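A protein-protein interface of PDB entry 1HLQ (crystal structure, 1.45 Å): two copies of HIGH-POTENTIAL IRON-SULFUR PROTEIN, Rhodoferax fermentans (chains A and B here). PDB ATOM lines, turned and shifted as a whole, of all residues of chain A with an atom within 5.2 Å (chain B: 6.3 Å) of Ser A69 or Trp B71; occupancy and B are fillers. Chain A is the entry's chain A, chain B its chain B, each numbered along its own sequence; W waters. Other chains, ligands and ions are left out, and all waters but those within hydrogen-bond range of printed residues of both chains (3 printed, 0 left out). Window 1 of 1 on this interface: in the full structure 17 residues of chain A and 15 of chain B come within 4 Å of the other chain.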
ATOM      1  N   LEU A  15     -27.350  -9.817  17.802  1.00  0.00           N
ATOM      2  CA  LEU A  15     -28.333 -10.413  18.687  1.00  0.00           C
ATOM      3  C   LEU A  15     -29.739 -10.443  18.113  1.00  0.00           C
ATOM      4  O   LEU A  15     -30.711 -10.755  18.814  1.00  0.00           O
ATOM      5  CB  LEU A  15     -28.351  -9.654  20.021  1.00  0.00           C
ATOM      6  CG  LEU A  15     -27.097  -9.803  20.888  1.00  0.00           C
ATOM      7  CD1 LEU A  15     -27.063  -8.795  22.010  1.00  0.00           C
ATOM      8  CD2 LEU A  15     -27.039 -11.219  21.452  1.00  0.00           C
ATOM      9  N   GLY A  16     -29.904 -10.102  16.837  1.00  0.00           N
ATOM     10  CA  GLY A  16     -31.227 -10.061  16.219  1.00  0.00           C
ATOM     11  C   GLY A  16     -32.169  -9.100  16.921  1.00  0.00           C
ATOM     12  O   GLY A  16     -33.378  -9.322  16.974  1.00  0.00           O
ATOM     13  N   TYR A  29     -35.008 -17.454  14.707  1.00  0.00           N
ATOM     14  CA  TYR A  29     -35.154 -17.727  16.135  1.00  0.00           C
ATOM     15  C   TYR A  29     -36.526 -18.350  16.401  1.00  0.00           C
ATOM     16  O   TYR A  29     -37.485 -17.689  16.810  1.00  0.00           O
ATOM     17  CB  TYR A  29     -35.004 -16.416  16.936  1.00  0.00           C
ATOM     18  CG  TYR A  29     -33.790 -15.572  16.588  1.00  0.00           C
ATOM     19  CD1 TYR A  29     -32.521 -15.943  16.986  1.00  0.00           C
ATOM     20  CD2 TYR A  29     -33.899 -14.426  15.815  1.00  0.00           C
ATOM     21  CE1 TYR A  29     -31.400 -15.204  16.661  1.00  0.00           C
ATOM     22  CE2 TYR A  29     -32.795 -13.667  15.473  1.00  0.00           C
ATOM     23  CZ  TYR A  29     -31.542 -14.067  15.895  1.00  0.00           C
ATOM     24  OH  TYR A  29     -30.457 -13.303  15.534  1.00  0.00           O
ATOM     25  N   TRP A  67     -37.046  -6.933  21.624  1.00  0.00           N
ATOM     26  CA  TRP A  67     -36.570  -8.288  21.857  1.00  0.00           C
ATOM     27  C   TRP A  67     -35.194  -8.470  21.231  1.00  0.00           C
ATOM     28  O   TRP A  67     -34.854  -7.854  20.234  1.00  0.00           O
ATOM     29  CB  TRP A  67     -37.530  -9.272  21.147  1.00  0.00           C
ATOM     30  CG  TRP A  67     -37.196 -10.722  21.321  1.00  0.00           C
ATOM     31  CD1 TRP A  67     -37.623 -11.540  22.322  1.00  0.00           C
ATOM     32  CD2 TRP A  67     -36.379 -11.531  20.475  1.00  0.00           C
ATOM     33  NE1 TRP A  67     -37.113 -12.813  22.176  1.00  0.00           N
ATOM     34  CE2 TRP A  67     -36.345 -12.831  21.037  1.00  0.00           C
ATOM     35  CE3 TRP A  67     -35.663 -11.300  19.295  1.00  0.00           C
ATOM     36  CZ2 TRP A  67     -35.624 -13.877  20.465  1.00  0.00           C
ATOM     37  CZ3 TRP A  67     -34.942 -12.339  18.732  1.00  0.00           C
ATOM     38  CH2 TRP A  67     -34.939 -13.610  19.311  1.00  0.00           C
ATOM     39  N   CYS A  68     -34.422  -9.363  21.842  1.00  0.00           N
ATOM     40  CA  CYS A  68     -33.173  -9.805  21.234  1.00  0.00           C
ATOM     41  C   CYS A  68     -32.976 -11.269  21.631  1.00  0.00           C
ATOM     42  O   CYS A  68     -33.692 -11.804  22.478  1.00  0.00           O
ATOM     43  CB  CYS A  68     -31.953  -8.959  21.526  1.00  0.00           C
ATOM     44  SG  CYS A  68     -31.110  -9.419  23.057  1.00  0.00           S
ATOM     45  N   SER A  69     -32.007 -11.903  20.971  1.00  0.00           N
ATOM     46  CA  SER A  69     -31.799 -13.341  21.145  1.00  0.00           C
ATOM     47  C   SER A  69     -31.363 -13.722  22.538  1.00  0.00           C
ATOM     48  O   SER A  69     -31.472 -14.903  22.900  1.00  0.00           O
ATOM     49  CB  SER A  69     -30.713 -13.724  20.121  1.00  0.00           C
ATOM     50  OG  SER A  69     -30.421 -15.099  20.111  1.00  0.00           O
ATOM     51  N   ALA A  70     -30.855 -12.806  23.346  1.00  0.00           N
ATOM     52  CA  ALA A  70     -30.474 -13.039  24.713  1.00  0.00           C
ATOM     53  C   ALA A  70     -31.640 -12.968  25.685  1.00  0.00           C
ATOM     54  O   ALA A  70     -31.421 -13.050  26.902  1.00  0.00           O
ATOM     55  CB  ALA A  70     -29.391 -12.044  25.144  1.00  0.00           C
ATOM     56  N   TRP A  71     -32.874 -12.765  25.178  1.00  0.00           N
ATOM     57  CA  TRP A  71     -34.015 -12.662  26.074  1.00  0.00           C
ATOM     58  C   TRP A  71     -33.942 -13.698  27.185  1.00  0.00           C
ATOM     59  O   TRP A  71     -33.844 -14.887  26.863  1.00  0.00           O
ATOM     60  CB  TRP A  71     -35.332 -12.779  25.302  1.00  0.00           C
ATOM     61  CG  TRP A  71     -36.501 -12.644  26.226  1.00  0.00           C
ATOM     62  CD1 TRP A  71     -37.106 -11.483  26.599  1.00  0.00           C
ATOM     63  CD2 TRP A  71     -37.197 -13.703  26.892  1.00  0.00           C
ATOM     64  NE1 TRP A  71     -38.118 -11.732  27.486  1.00  0.00           N
ATOM     65  CE2 TRP A  71     -38.208 -13.098  27.672  1.00  0.00           C
ATOM     66  CE3 TRP A  71     -37.062 -15.097  26.907  1.00  0.00           C
ATOM     67  CZ2 TRP A  71     -39.082 -13.824  28.468  1.00  0.00           C
ATOM     68  CZ3 TRP A  71     -37.942 -15.808  27.696  1.00  0.00           C
ATOM     69  CH2 TRP A  71     -38.933 -15.178  28.452  1.00  0.00           C
ATOM     70  N   ASP B  35     -28.209 -28.558  22.820  1.00  0.00           N
ATOM     71  CA  ASP B  35     -27.546 -27.950  21.690  1.00  0.00           C
ATOM     72  C   ASP B  35     -27.157 -26.509  22.007  1.00  0.00           C
ATOM     73  O   ASP B  35     -26.364 -25.907  21.279  1.00  0.00           O
ATOM     74  CB  ASP B  35     -28.443 -28.009  20.455  1.00  0.00           C
ATOM     75  CG  ASP B  35     -28.748 -29.428  20.043  1.00  0.00           C
ATOM     76  OD1 ASP B  35     -29.931 -29.805  20.007  1.00  0.00           O
ATOM     77  OD2 ASP B  35     -27.770 -30.173  19.811  1.00  0.00           O
ATOM     78  N   GLN B  36     -27.689 -25.969  23.104  1.00  0.00           N
ATOM     79  CA  GLN B  36     -27.382 -24.640  23.579  1.00  0.00           C
ATOM     80  C   GLN B  36     -26.293 -24.729  24.646  1.00  0.00           C
ATOM     81  O   GLN B  36     -26.398 -25.427  25.665  1.00  0.00           O
ATOM     82  CB  GLN B  36     -28.587 -23.952  24.231  1.00  0.00           C
ATOM     83  CG  GLN B  36     -29.806 -23.903  23.355  1.00  0.00           C
ATOM     84  CD  GLN B  36     -31.016 -23.277  24.015  1.00  0.00           C
ATOM     85  OE1 GLN B  36     -30.947 -22.785  25.140  1.00  0.00           O
ATOM     86  NE2 GLN B  36     -32.131 -23.363  23.307  1.00  0.00           N
ATOM     87  N   SER B  37     -25.214 -24.003  24.431  1.00  0.00           N
ATOM     88  CA  SER B  37     -24.158 -23.893  25.411  1.00  0.00           C
ATOM     89  C   SER B  37     -23.411 -22.596  25.154  1.00  0.00           C
ATOM     90  O   SER B  37     -23.557 -22.027  24.068  1.00  0.00           O
ATOM     91  CB  SER B  37     -23.218 -25.099  25.318  1.00  0.00           C
ATOM     92  OG  SER B  37     -22.729 -25.313  23.995  1.00  0.00           O
ATOM     93  N   CYS B  38     -22.596 -22.150  26.095  1.00  0.00           N
ATOM     94  CA  CYS B  38     -21.792 -20.953  25.883  1.00  0.00           C
ATOM     95  C   CYS B  38     -21.006 -21.040  24.586  1.00  0.00           C
ATOM     96  O   CYS B  38     -20.887 -20.039  23.881  1.00  0.00           O
ATOM     97  CB  CYS B  38     -20.849 -20.728  27.058  1.00  0.00           C
ATOM     98  SG  CYS B  38     -21.661 -20.659  28.654  1.00  0.00           S
ATOM     99  N   SER B  39     -20.501 -22.204  24.197  1.00  0.00           N
ATOM    100  CA  SER B  39     -19.800 -22.380  22.947  1.00  0.00           C
ATOM    101  C   SER B  39     -20.555 -21.887  21.721  1.00  0.00           C
ATOM    102  O   SER B  39     -19.894 -21.512  20.749  1.00  0.00           O
ATOM    103  CB  SER B  39     -19.457 -23.855  22.720  1.00  0.00           C
ATOM    104  OG  SER B  39     -20.583 -24.679  22.492  1.00  0.00           O
ATOM    105  N   THR B  40     -21.884 -21.940  21.739  1.00  0.00           N
ATOM    106  CA  THR B  40     -22.674 -21.515  20.594  1.00  0.00           C
ATOM    107  C   THR B  40     -23.426 -20.218  20.887  1.00  0.00           C
ATOM    108  O   THR B  40     -24.323 -19.853  20.112  1.00  0.00           O
ATOM    109  CB  THR B  40     -23.664 -22.620  20.168  1.00  0.00           C
ATOM    110  OG1 THR B  40     -24.504 -22.969  21.279  1.00  0.00           O
ATOM    111  CG2 THR B  40     -22.947 -23.874  19.689  1.00  0.00           C
ATOM    112  N   CYS B  41     -23.118 -19.555  21.978  1.00  0.00           N
ATOM    113  CA  CYS B  41     -23.800 -18.318  22.376  1.00  0.00           C
ATOM    114  C   CYS B  41     -23.141 -17.105  21.736  1.00  0.00           C
ATOM    115  O   CYS B  41     -21.922 -16.975  21.789  1.00  0.00           O
ATOM    116  CB  CYS B  41     -23.708 -18.129  23.895  1.00  0.00           C
ATOM    117  SG  CYS B  41     -24.534 -16.676  24.586  1.00  0.00           S
ATOM    118  N   ALA B  42     -23.971 -16.163  21.294  1.00  0.00           N
ATOM    119  CA  ALA B  42     -23.469 -14.937  20.671  1.00  0.00           C
ATOM    120  C   ALA B  42     -22.747 -14.052  21.650  1.00  0.00           C
ATOM    121  O   ALA B  42     -22.053 -13.115  21.226  1.00  0.00           O
ATOM    122  CB  ALA B  42     -24.648 -14.186  20.048  1.00  0.00           C
ATOM    123  N   LEU B  43     -22.855 -14.205  22.959  1.00  0.00           N
ATOM    124  CA  LEU B  43     -22.175 -13.388  23.935  1.00  0.00           C
ATOM    125  C   LEU B  43     -20.842 -13.991  24.395  1.00  0.00           C
ATOM    126  O   LEU B  43     -20.046 -13.235  24.959  1.00  0.00           O
ATOM    127  CB  LEU B  43     -23.073 -13.118  25.139  1.00  0.00           C
ATOM    128  CG  LEU B  43     -24.406 -12.427  24.779  1.00  0.00           C
ATOM    129  CD1 LEU B  43     -25.241 -12.298  26.026  1.00  0.00           C
ATOM    130  CD2 LEU B  43     -24.137 -11.050  24.191  1.00  0.00           C
ATOM    131  N   GLY B  66     -21.141 -25.021  29.290  1.00  0.00           N
ATOM    132  CA  GLY B  66     -22.112 -24.435  30.173  1.00  0.00           C
ATOM    133  C   GLY B  66     -23.277 -23.706  29.503  1.00  0.00           C
ATOM    134  O   GLY B  66     -23.458 -23.822  28.294  1.00  0.00           O
ATOM    135  N   TRP B  67     -24.133 -23.104  30.319  1.00  0.00           N
ATOM    136  CA  TRP B  67     -25.323 -22.428  29.808  1.00  0.00           C
ATOM    137  C   TRP B  67     -25.966 -21.515  30.830  1.00  0.00           C
ATOM    138  O   TRP B  67     -25.886 -21.741  32.045  1.00  0.00           O
ATOM    139  CB  TRP B  67     -26.372 -23.524  29.504  1.00  0.00           C
ATOM    140  CG  TRP B  67     -27.680 -23.070  28.929  1.00  0.00           C
ATOM    141  CD1 TRP B  67     -27.972 -22.951  27.599  1.00  0.00           C
ATOM    142  CD2 TRP B  67     -28.874 -22.715  29.633  1.00  0.00           C
ATOM    143  NE1 TRP B  67     -29.279 -22.553  27.442  1.00  0.00           N
ATOM    144  CE2 TRP B  67     -29.846 -22.369  28.678  1.00  0.00           C
ATOM    145  CE3 TRP B  67     -29.233 -22.632  30.995  1.00  0.00           C
ATOM    146  CZ2 TRP B  67     -31.146 -21.961  29.007  1.00  0.00           C
ATOM    147  CZ3 TRP B  67     -30.508 -22.231  31.321  1.00  0.00           C
ATOM    148  CH2 TRP B  67     -31.452 -21.894  30.337  1.00  0.00           C
ATOM    149  N   CYS B  68     -26.673 -20.480  30.377  1.00  0.00           N
ATOM    150  CA  CYS B  68     -27.493 -19.645  31.244  1.00  0.00           C
ATOM    151  C   CYS B  68     -28.737 -19.210  30.445  1.00  0.00           C
ATOM    152  O   CYS B  68     -28.810 -19.424  29.239  1.00  0.00           O
ATOM    153  CB  CYS B  68     -26.861 -18.442  31.908  1.00  0.00           C
ATOM    154  SG  CYS B  68     -26.794 -16.987  30.850  1.00  0.00           S
ATOM    155  N   SER B  69     -29.743 -18.665  31.123  1.00  0.00           N
ATOM    156  CA  SER B  69     -31.007 -18.341  30.465  1.00  0.00           C
ATOM    157  C   SER B  69     -30.914 -17.276  29.392  1.00  0.00           C
ATOM    158  O   SER B  69     -31.833 -17.160  28.563  1.00  0.00           O
ATOM    159  CB  SER B  69     -32.095 -17.959  31.456  1.00  0.00           C
ATOM    160  OG  SER B  69     -31.743 -16.797  32.171  1.00  0.00           O
ATOM    161  N   ALA B  70     -29.815 -16.530  29.385  1.00  0.00           N
ATOM    162  CA  ALA B  70     -29.593 -15.520  28.357  1.00  0.00           C
ATOM    163  C   ALA B  70     -28.924 -16.093  27.113  1.00  0.00           C
ATOM    164  O   ALA B  70     -28.599 -15.355  26.175  1.00  0.00           O
ATOM    165  CB  ALA B  70     -28.749 -14.357  28.871  1.00  0.00           C
ATOM    166  N   TRP B  71     -28.735 -17.408  27.042  1.00  0.00           N
ATOM    167  CA  TRP B  71     -28.118 -18.056  25.897  1.00  0.00           C
ATOM    168  C   TRP B  71     -28.694 -17.441  24.626  1.00  0.00           C
ATOM    169  O   TRP B  71     -29.911 -17.470  24.426  1.00  0.00           O
ATOM    170  CB  TRP B  71     -28.317 -19.578  25.900  1.00  0.00           C
ATOM    171  CG  TRP B  71     -27.688 -20.203  24.677  1.00  0.00           C
ATOM    172  CD1 TRP B  71     -26.372 -20.536  24.529  1.00  0.00           C
ATOM    173  CD2 TRP B  71     -28.333 -20.449  23.431  1.00  0.00           C
ATOM    174  NE1 TRP B  71     -26.167 -21.021  23.266  1.00  0.00           N
ATOM    175  CE2 TRP B  71     -27.336 -20.976  22.559  1.00  0.00           C
ATOM    176  CE3 TRP B  71     -29.627 -20.311  22.950  1.00  0.00           C
ATOM    177  CZ2 TRP B  71     -27.625 -21.372  21.258  1.00  0.00           C
ATOM    178  CZ3 TRP B  71     -29.920 -20.719  21.658  1.00  0.00           C
ATOM    179  CH2 TRP B  71     -28.914 -21.234  20.828  1.00  0.00           C
ATOM    180  N   ALA B  72     -27.792 -16.970  23.773  1.00  0.00           N
ATOM    181  CA  ALA B  72     -28.210 -16.207  22.598  1.00  0.00           C
ATOM    182  C   ALA B  72     -27.794 -16.854  21.301  1.00  0.00           C
ATOM    183  O   ALA B  72     -26.598 -16.902  20.956  1.00  0.00           O
ATOM    184  CB  ALA B  72     -27.542 -14.843  22.774  1.00  0.00           C
ATOM    185  N   LYS B  73     -28.754 -17.426  20.593  1.00  0.00           N
ATOM    186  CA  LYS B  73     -28.501 -18.047  19.306  1.00  0.00           C
ATOM    187  C   LYS B  73     -27.820 -17.019  18.403  1.00  0.00           C
ATOM    188  O   LYS B  73     -28.227 -15.856  18.377  1.00  0.00           O
ATOM    189  CB  LYS B  73     -29.795 -18.552  18.680  1.00  0.00           C
ATOM    190  CG  LYS B  73     -29.614 -19.275  17.356  1.00  0.00           C
ATOM    191  CD  LYS B  73     -30.955 -19.769  16.822  1.00  0.00           C
ATOM    192  CE  LYS B  73     -30.718 -20.423  15.458  1.00  0.00           C
ATOM    193  NZ  LYS B  73     -31.986 -20.969  14.919  1.00  0.00           N
ATOM    194  N   LYS B  74     -26.782 -17.445  17.704  1.00  0.00           N
ATOM    195  CA  LYS B  74     -26.057 -16.514  16.832  1.00  0.00           C
ATOM    196  C   LYS B  74     -26.817 -16.144  15.576  1.00  0.00           C
ATOM    197  O   LYS B  74     -27.647 -16.898  15.079  1.00  0.00           O
ATOM    198  CB  LYS B  74     -24.716 -17.160  16.447  1.00  0.00           C
ATOM    199  CG  LYS B  74     -23.748 -17.234  17.612  1.00  0.00           C
ATOM    200  CD  LYS B  74     -22.507 -18.018  17.187  1.00  0.00           C
ATOM    201  CE  LYS B  74     -21.506 -18.006  18.334  1.00  0.00           C
ATOM    202  NZ  LYS B  74     -20.231 -18.654  17.937  1.00  0.00           N
HETATM  203  O   HOH W   1     -34.489 -17.303  28.386  1.00  0.00           O
HETATM  204  O   HOH W   2     -28.516 -13.458  17.331  1.00  0.00           O
HETATM  205  O   HOH W   3     -31.433 -17.465  21.942  1.00  0.00           O
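The side-chain hydroxyl (OG) of Ser A69 lies within hydrogen-bond range of the backbone carbonyl oxygen (O) of Lys B73. The backbone carbonyl oxygen of Ser A69 sits close to the backbone carbonyl oxygen of Trp B71, at 3.4 Å. O of Ser B69 sits close to O of Trp A71.
N of Ser A69 sits at hydrogen-bond distance from O of Leu A15 (2.8 Å). O of Ser B37 is in hydrogen-bond range of NE1 of Trp B71 (2.9 Å). The side-chain hydroxyl (OG1) of Thr B40 lies within hydrogen-bond range of the indole nitrogen (NE1) of Trp B71. N of Leu B43 lies close to SG of Cys B41. The backbone NH (N) of Ala B72 sits close to the side-chain sulfur (SG) of Cys B41, at 3.4 Å. The backbone NH (N) of Ala B42 is in hydrogen-bond range of the backbone carbonyl oxygen (O) of Ala B72 (2.7 Å).
Among the printed residues, pairs that only touch across the chains: Leu A15 with Leu B43 (3.99 Å), Leu A15 with Ala B72 (3.9 Å), Tyr A29 with Lys B73 (3.7 Å), Ser A69 with Ala B72 (3.4 Å), Ala A70 with Ala B70 (3.3 Å) and Ala A70 with Ala B72 (3.9 Å).
Of the printed residues of chain B, Ser A69 touches Trp B71, Ala B72 and Lys B73. Printed residues of chain A within 4 Å of Trp B71: Ser A69 (3.4 Å). Printed residues of chain A within 4 Å of Ser B69: Trp A71 (3.5 Å). Printed residues of chain A within 4 Å of Leu B43: Leu A15. Printed residues of chain B within 4 Å of Trp A71: Ser B69. Printed residues of chain A within 4 Å of Lys B73: Tyr A29 and Ser A69. Of the printed residues of chain A, Ala B72 touches Leu A15 (3.9 Å), Ser A69 (3.4 Å) and Ala A70 (3.9 Å). The nearest printed residue of chain B that does not touch Trp A71 is Ala B70 (4.6 Å).
Hydrophobic or aromatic side chains of chain B that line the printed part of chain A: Leu B43, Ala B70 and Ala B72. Along chain B the printed residues that touch a printed residue of chain A span positions 43 to 73. Of the 8 printed residues of chain A, 5 touch a printed residue of chain B. Hydrophobic or aromatic side chains of chain A that line the printed part of chain B: Leu A15, Tyr A29 and Ala A70.
Ser A69 touches Trp B71, and with the chains exchanged Trp A71 touches Ser B69. Ala B70 touches its own counterpart, Ala A70. 5 positions are printed for both chains. Of the 9 pairs that touch across the chains among the printed residues, 3 have their exchanged pair printed and touching as well.
Water W2 bridges the backbone carbonyl oxygen of Lys B73 and the side-chain hydroxyl of Tyr A29. Water W1 lies within hydrogen-bond range of O of Ser B69 (2.7 Å) and O of Trp A71 (2.9 Å). Water W3 lies within hydrogen-bond range of O of Ser A69, O of Trp B71 and N of Lys B73.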
